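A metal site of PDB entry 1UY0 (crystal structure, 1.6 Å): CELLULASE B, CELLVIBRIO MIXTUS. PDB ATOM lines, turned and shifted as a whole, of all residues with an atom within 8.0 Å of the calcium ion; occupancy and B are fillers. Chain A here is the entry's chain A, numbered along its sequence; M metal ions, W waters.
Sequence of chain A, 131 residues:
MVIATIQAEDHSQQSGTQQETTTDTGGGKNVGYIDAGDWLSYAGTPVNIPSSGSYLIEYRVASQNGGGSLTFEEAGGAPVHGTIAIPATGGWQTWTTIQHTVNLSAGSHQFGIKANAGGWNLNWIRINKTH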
ATOM      1  N   ILE A   6     -12.282 -19.789   7.294  1.00  0.00           N
ATOM      2  CA  ILE A   6     -11.172 -20.744   7.175  1.00  0.00           C
ATOM      3  C   ILE A   6     -11.144 -21.281   5.745  1.00  0.00           C
ATOM      4  O   ILE A   6     -12.088 -21.899   5.281  1.00  0.00           O
ATOM      5  CB  ILE A   6     -11.377 -21.875   8.133  1.00  0.00           C
ATOM      6  CG1 ILE A   6     -11.228 -21.408   9.594  1.00  0.00           C
ATOM      7  CG2 ILE A   6     -10.401 -23.028   7.884  1.00  0.00           C
ATOM      8  CD1 ILE A   6     -11.704 -22.464  10.578  1.00  0.00           C
ATOM      9  N   GLN A   7     -10.069 -21.021   5.031  1.00  0.00           N
ATOM     10  CA  GLN A   7      -9.902 -21.639   3.729  1.00  0.00           C
ATOM     11  C   GLN A   7      -9.713 -23.138   3.922  1.00  0.00           C
ATOM     12  O   GLN A   7      -8.925 -23.554   4.759  1.00  0.00           O
ATOM     13  CB  GLN A   7      -8.710 -21.034   3.005  1.00  0.00           C
ATOM     14  CG  GLN A   7      -8.949 -19.557   2.594  1.00  0.00           C
ATOM     15  CD  GLN A   7     -10.125 -19.395   1.651  1.00  0.00           C
ATOM     16  OE1 GLN A   7     -10.333 -20.222   0.752  1.00  0.00           O
ATOM     17  NE2 GLN A   7     -10.888 -18.306   1.827  1.00  0.00           N
ATOM     18  N   ALA A   8     -10.407 -23.946   3.126  1.00  0.00           N
ATOM     19  CA  ALA A   8     -10.447 -25.397   3.380  1.00  0.00           C
ATOM     20  C   ALA A   8      -9.087 -26.055   3.239  1.00  0.00           C
ATOM     21  O   ALA A   8      -8.805 -27.038   3.937  1.00  0.00           O
ATOM     22  CB  ALA A   8     -11.457 -26.047   2.493  1.00  0.00           C
ATOM     23  N   GLU A   9      -8.257 -25.502   2.372  1.00  0.00           N
ATOM     24  CA  GLU A   9      -6.926 -26.008   2.149  1.00  0.00           C
ATOM     25  C   GLU A   9      -5.967 -25.694   3.308  1.00  0.00           C
ATOM     26  O   GLU A   9      -4.903 -26.301   3.403  1.00  0.00           O
ATOM     27  CB  GLU A   9      -6.375 -25.474   0.820  1.00  0.00           C
ATOM     28  CG  GLU A   9      -6.033 -23.988   0.788  1.00  0.00           C
ATOM     29  CD  GLU A   9      -7.178 -23.079   0.403  1.00  0.00           C
ATOM     30  OE1 GLU A   9      -8.377 -23.452   0.513  1.00  0.00           O
ATOM     31  OE2 GLU A   9      -6.878 -21.944  -0.032  1.00  0.00           O
ATOM     32  N   ASP A  10      -6.358 -24.778   4.199  1.00  0.00           N
ATOM     33  CA  ASP A  10      -5.487 -24.338   5.302  1.00  0.00           C
ATOM     34  C   ASP A  10      -5.663 -25.220   6.526  1.00  0.00           C
ATOM     35  O   ASP A  10      -5.735 -24.767   7.669  1.00  0.00           O
ATOM     36  CB  ASP A  10      -5.748 -22.881   5.636  1.00  0.00           C
ATOM     37  CG  ASP A  10      -5.218 -21.937   4.585  1.00  0.00           C
ATOM     38  OD1 ASP A  10      -4.466 -22.377   3.673  1.00  0.00           O
ATOM     39  OD2 ASP A  10      -5.512 -20.715   4.597  1.00  0.00           O
ATOM     40  N   GLN A  19      -5.399 -30.834  -2.712  1.00  0.00           N
ATOM     41  CA  GLN A  19      -5.809 -29.490  -3.121  1.00  0.00           C
ATOM     42  C   GLN A  19      -5.688 -29.330  -4.640  1.00  0.00           C
ATOM     43  O   GLN A  19      -4.982 -30.056  -5.316  1.00  0.00           O
ATOM     44  CB  GLN A  19      -5.038 -28.375  -2.390  1.00  0.00           C
ATOM     45  CG  GLN A  19      -3.604 -28.195  -2.732  1.00  0.00           C
ATOM     46  CD  GLN A  19      -3.025 -26.861  -2.186  1.00  0.00           C
ATOM     47  OE1 GLN A  19      -2.159 -26.264  -2.847  1.00  0.00           O
ATOM     48  NE2 GLN A  19      -3.482 -26.406  -1.013  1.00  0.00           N
ATOM     49  N   GLU A  20      -6.432 -28.376  -5.147  1.00  0.00           N
ATOM     50  CA  GLU A  20      -6.418 -28.066  -6.568  1.00  0.00           C
ATOM     51  C   GLU A  20      -6.820 -26.621  -6.732  1.00  0.00           C
ATOM     52  O   GLU A  20      -7.430 -26.009  -5.854  1.00  0.00           O
ATOM     53  CB  GLU A  20      -7.333 -28.992  -7.340  1.00  0.00           C
ATOM     54  CG  GLU A  20      -8.795 -28.897  -6.955  1.00  0.00           C
ATOM     55  CD  GLU A  20      -9.665 -30.003  -7.498  1.00  0.00           C
ATOM     56  OE1 GLU A  20      -9.180 -30.834  -8.314  1.00  0.00           O
ATOM     57  OE2 GLU A  20     -10.884 -30.010  -7.154  1.00  0.00           O
ATOM     58  N   THR A  22      -8.864 -23.462  -7.751  1.00  0.00           N
ATOM     59  CA  THR A  22     -10.285 -23.181  -7.933  1.00  0.00           C
ATOM     60  C   THR A  22     -10.477 -21.977  -8.833  1.00  0.00           C
ATOM     61  O   THR A  22      -9.668 -21.039  -8.783  1.00  0.00           O
ATOM     62  CB  THR A  22     -11.021 -22.959  -6.584  1.00  0.00           C
ATOM     63  OG1 THR A  22     -12.424 -22.806  -6.818  1.00  0.00           O
ATOM     64  CG2 THR A  22     -10.596 -21.669  -5.844  1.00  0.00           C
ATOM     65  N   ASP A  24     -13.488 -20.475  -8.521  1.00  0.00           N
ATOM     66  CA  ASP A  24     -14.428 -19.679  -7.738  1.00  0.00           C
ATOM     67  C   ASP A  24     -13.930 -18.238  -7.548  1.00  0.00           C
ATOM     68  O   ASP A  24     -12.737 -17.962  -7.691  1.00  0.00           O
ATOM     69  CB  ASP A  24     -14.639 -20.331  -6.357  1.00  0.00           C
ATOM     70  CG  ASP A  24     -15.869 -19.843  -5.659  1.00  0.00           C
ATOM     71  OD1 ASP A  24     -16.777 -19.234  -6.304  1.00  0.00           O
ATOM     72  OD2 ASP A  24     -16.026 -20.057  -4.435  1.00  0.00           O
ATOM     73  N   THR A  25     -14.846 -17.342  -7.228  1.00  0.00           N
ATOM     74  CA  THR A  25     -14.511 -15.978  -6.857  1.00  0.00           C
ATOM     75  C   THR A  25     -13.397 -15.905  -5.818  1.00  0.00           C
ATOM     76  O   THR A  25     -13.473 -16.561  -4.765  1.00  0.00           O
ATOM     77  CB  THR A  25     -15.746 -15.266  -6.290  1.00  0.00           C
ATOM     78  OG1 THR A  25     -16.877 -15.520  -7.127  1.00  0.00           O
ATOM     79  CG2 THR A  25     -15.564 -13.758  -6.325  1.00  0.00           C
ATOM     80  N   GLY A  26     -12.371 -15.094  -6.112  1.00  0.00           N
ATOM     81  CA  GLY A  26     -11.211 -14.951  -5.243  1.00  0.00           C
ATOM     82  C   GLY A  26     -10.051 -15.870  -5.596  1.00  0.00           C
ATOM     83  O   GLY A  26      -8.944 -15.701  -5.059  1.00  0.00           O
ATOM     84  N   GLY A  27     -10.302 -16.849  -6.464  1.00  0.00           N
ATOM     85  CA  GLY A  27      -9.283 -17.794  -6.863  1.00  0.00           C
ATOM     86  C   GLY A  27      -8.735 -18.581  -5.671  1.00  0.00           C
ATOM     87  O   GLY A  27      -9.444 -18.832  -4.691  1.00  0.00           O
ATOM     88  N   GLY A  28      -7.459 -18.932  -5.746  1.00  0.00           N
ATOM     89  CA  GLY A  28      -6.839 -19.740  -4.717  1.00  0.00           C
ATOM     90  C   GLY A  28      -7.007 -21.234  -4.967  1.00  0.00           C
ATOM     91  O   GLY A  28      -6.870 -21.715  -6.102  1.00  0.00           O
ATOM     92  N   LYS A  29      -7.285 -21.981  -3.899  1.00  0.00           N
ATOM     93  CA  LYS A  29      -7.385 -23.432  -3.983  1.00  0.00           C
ATOM     94  C   LYS A  29      -8.635 -23.956  -3.315  1.00  0.00           C
ATOM     95  O   LYS A  29      -9.196 -23.316  -2.426  1.00  0.00           O
ATOM     96  CB  LYS A  29      -6.206 -24.065  -3.254  1.00  0.00           C
ATOM     97  CG  LYS A  29      -4.818 -23.615  -3.715  1.00  0.00           C
ATOM     98  CD  LYS A  29      -4.517 -24.131  -5.066  1.00  0.00           C
ATOM     99  CE  LYS A  29      -3.043 -23.889  -5.465  1.00  0.00           C
ATOM    100  NZ  LYS A  29      -2.899 -24.125  -6.913  1.00  0.00           N
ATOM    101  N   ASN A  30      -9.062 -25.135  -3.730  1.00  0.00           N
ATOM    102  CA  ASN A  30     -10.065 -25.879  -2.980  1.00  0.00           C
ATOM    103  C   ASN A  30      -9.535 -27.253  -2.653  1.00  0.00           C
ATOM    104  O   ASN A  30      -8.573 -27.717  -3.233  1.00  0.00           O
ATOM    105  CB  ASN A  30     -11.387 -25.954  -3.750  1.00  0.00           C
ATOM    106  CG  ASN A  30     -11.327 -26.833  -4.989  1.00  0.00           C
ATOM    107  OD1 ASN A  30     -11.513 -28.092  -4.921  1.00  0.00           O
ATOM    108  ND2 ASN A  30     -11.134 -26.215  -6.118  1.00  0.00           N
ATOM    109  N   VAL A  31     -10.195 -27.892  -1.707  1.00  0.00           N
ATOM    110  CA  VAL A  31      -9.964 -29.303  -1.421  1.00  0.00           C
ATOM    111  C   VAL A  31     -10.817 -30.137  -2.344  1.00  0.00           C
ATOM    112  O   VAL A  31     -11.995 -29.880  -2.546  1.00  0.00           O
ATOM    113  CB  VAL A  31     -10.301 -29.612   0.021  1.00  0.00           C
ATOM    114  CG1 VAL A  31     -10.109 -31.127   0.284  1.00  0.00           C
ATOM    115  CG2 VAL A  31      -9.416 -28.809   0.948  1.00  0.00           C
ATOM    116  N   ARG A  60     -18.562 -23.401   1.346  1.00  0.00           N
ATOM    117  CA  ARG A  60     -18.497 -23.059  -0.078  1.00  0.00           C
ATOM    118  C   ARG A  60     -18.126 -24.325  -0.815  1.00  0.00           C
ATOM    119  O   ARG A  60     -17.001 -24.785  -0.715  1.00  0.00           O
ATOM    120  CB  ARG A  60     -17.460 -21.975  -0.298  1.00  0.00           C
ATOM    121  CG  ARG A  60     -17.428 -21.374  -1.705  1.00  0.00           C
ATOM    122  CD  ARG A  60     -18.729 -20.684  -2.059  1.00  0.00           C
ATOM    123  NE  ARG A  60     -18.609 -19.973  -3.322  1.00  0.00           N
ATOM    124  CZ  ARG A  60     -19.611 -19.321  -3.909  1.00  0.00           C
ATOM    125  NH1 ARG A  60     -20.802 -19.271  -3.342  1.00  0.00           N
ATOM    126  NH2 ARG A  60     -19.388 -18.711  -5.073  1.00  0.00           N
ATOM    127  N   TRP A  95     -19.913 -23.225  -7.978  1.00  0.00           N
ATOM    128  CA  TRP A  95     -19.855 -23.046  -6.522  1.00  0.00           C
ATOM    129  C   TRP A  95     -21.129 -22.472  -5.956  1.00  0.00           C
ATOM    130  O   TRP A  95     -21.810 -21.644  -6.582  1.00  0.00           O
ATOM    131  CB  TRP A  95     -18.682 -22.140  -6.157  1.00  0.00           C
ATOM    132  CG  TRP A  95     -17.401 -22.812  -6.517  1.00  0.00           C
ATOM    133  CD1 TRP A  95     -16.702 -22.692  -7.674  1.00  0.00           C
ATOM    134  CD2 TRP A  95     -16.680 -23.771  -5.717  1.00  0.00           C
ATOM    135  NE1 TRP A  95     -15.583 -23.481  -7.637  1.00  0.00           N
ATOM    136  CE2 TRP A  95     -15.551 -24.179  -6.452  1.00  0.00           C
ATOM    137  CE3 TRP A  95     -16.880 -24.322  -4.438  1.00  0.00           C
ATOM    138  CZ2 TRP A  95     -14.628 -25.093  -5.973  1.00  0.00           C
ATOM    139  CZ3 TRP A  95     -15.981 -25.249  -3.971  1.00  0.00           C
ATOM    140  CH2 TRP A  95     -14.849 -25.609  -4.726  1.00  0.00           C
ATOM    141  N   LEU A 122     -14.571 -28.495  -1.646  1.00  0.00           N
ATOM    142  CA  LEU A 122     -14.760 -27.539  -0.570  1.00  0.00           C
ATOM    143  C   LEU A 122     -13.734 -26.401  -0.679  1.00  0.00           C
ATOM    144  O   LEU A 122     -12.541 -26.632  -0.688  1.00  0.00           O
ATOM    145  CB  LEU A 122     -14.646 -28.215   0.793  1.00  0.00           C
ATOM    146  CG  LEU A 122     -14.916 -27.344   2.019  1.00  0.00           C
ATOM    147  CD1 LEU A 122     -16.341 -26.932   2.100  1.00  0.00           C
ATOM    148  CD2 LEU A 122     -14.536 -28.088   3.292  1.00  0.00           C
ATOM    149  N   ASN A 123     -14.196 -25.164  -0.773  1.00  0.00           N
ATOM    150  CA  ASN A 123     -13.314 -23.991  -0.932  1.00  0.00           C
ATOM    151  C   ASN A 123     -12.944 -23.345   0.396  1.00  0.00           C
ATOM    152  O   ASN A 123     -11.773 -23.060   0.658  1.00  0.00           O
ATOM    153  CB  ASN A 123     -13.978 -22.958  -1.871  1.00  0.00           C
ATOM    154  CG  ASN A 123     -13.048 -21.837  -2.302  1.00  0.00           C
ATOM    155  OD1 ASN A 123     -11.869 -21.811  -1.960  1.00  0.00           O
ATOM    156  ND2 ASN A 123     -13.611 -20.860  -3.041  1.00  0.00           N
ATOM    157  N   TRP A 124     -13.957 -23.108   1.225  1.00  0.00           N
ATOM    158  CA  TRP A 124     -13.783 -22.493   2.529  1.00  0.00           C
ATOM    159  C   TRP A 124     -14.989 -22.756   3.418  1.00  0.00           C
ATOM    160  O   TRP A 124     -16.036 -23.221   2.931  1.00  0.00           O
ATOM    161  CB  TRP A 124     -13.513 -20.978   2.416  1.00  0.00           C
ATOM    162  CG  TRP A 124     -14.446 -20.156   1.543  1.00  0.00           C
ATOM    163  CD1 TRP A 124     -14.163 -19.678   0.287  1.00  0.00           C
ATOM    164  CD2 TRP A 124     -15.782 -19.690   1.851  1.00  0.00           C
ATOM    165  NE1 TRP A 124     -15.237 -18.975  -0.203  1.00  0.00           N
ATOM    166  CE2 TRP A 124     -16.226 -18.932   0.735  1.00  0.00           C
ATOM    167  CE3 TRP A 124     -16.633 -19.802   2.953  1.00  0.00           C
ATOM    168  CZ2 TRP A 124     -17.474 -18.346   0.691  1.00  0.00           C
ATOM    169  CZ3 TRP A 124     -17.871 -19.219   2.910  1.00  0.00           C
ATOM    170  CH2 TRP A 124     -18.293 -18.499   1.766  1.00  0.00           C
ATOM    171  N   ILE A 125     -14.814 -22.475   4.709  1.00  0.00           N
ATOM    172  CA  ILE A 125     -15.861 -22.558   5.712  1.00  0.00           C
ATOM    173  C   ILE A 125     -15.917 -21.245   6.456  1.00  0.00           C
ATOM    174  O   ILE A 125     -14.914 -20.566   6.633  1.00  0.00           O
ATOM    175  CB  ILE A 125     -15.667 -23.749   6.687  1.00  0.00           C
ATOM    176  CG1 ILE A 125     -14.508 -23.566   7.614  1.00  0.00           C
ATOM    177  CG2 ILE A 125     -15.469 -25.006   5.922  1.00  0.00           C
ATOM    178  CD1 ILE A 125     -14.455 -24.652   8.697  1.00  0.00           C
HETATM  179 CA    CA M   1      -9.999 -22.010  -0.673  1.00  0.00          CA
HETATM  180  O   HOH W   1      -8.689 -20.220  -1.839  1.00  0.00           O
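The calcium ion is bound by OD1 of Asn 123 (2.3 Å), OE1 of Gln 7 (2.3 Å), O of Lys 29 (2.3 Å), O of Asn 123 (2.5 Å), OE1 of Glu 9 (2.5 Å) and water W1 (2.5 Å). The calcium ion has six donor atoms within binding distance.
The backbone NH (N) of Ala 8 lies close to the backbone carbonyl oxygen (O) of Asn 123. OD2 of Asp 24 lies within hydrogen-bond range of ND2 of Asn 123, 2.9 Å away. O of Arg 60 sits at hydrogen-bond distance from N of Asn 123.
Four residues have an atom within 4 Å of the calcium ion: Gln 7, Glu 9, Lys 29 and Asn 123. The nearest printed residue that does not touch the calcium ion is Ala 8 (4.3 Å).
Water W1 lies within hydrogen-bond range of the backbone NH of Lys 29, the side-chain carboxylate of Glu 9 and the backbone carbonyl oxygen of Gly 27.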
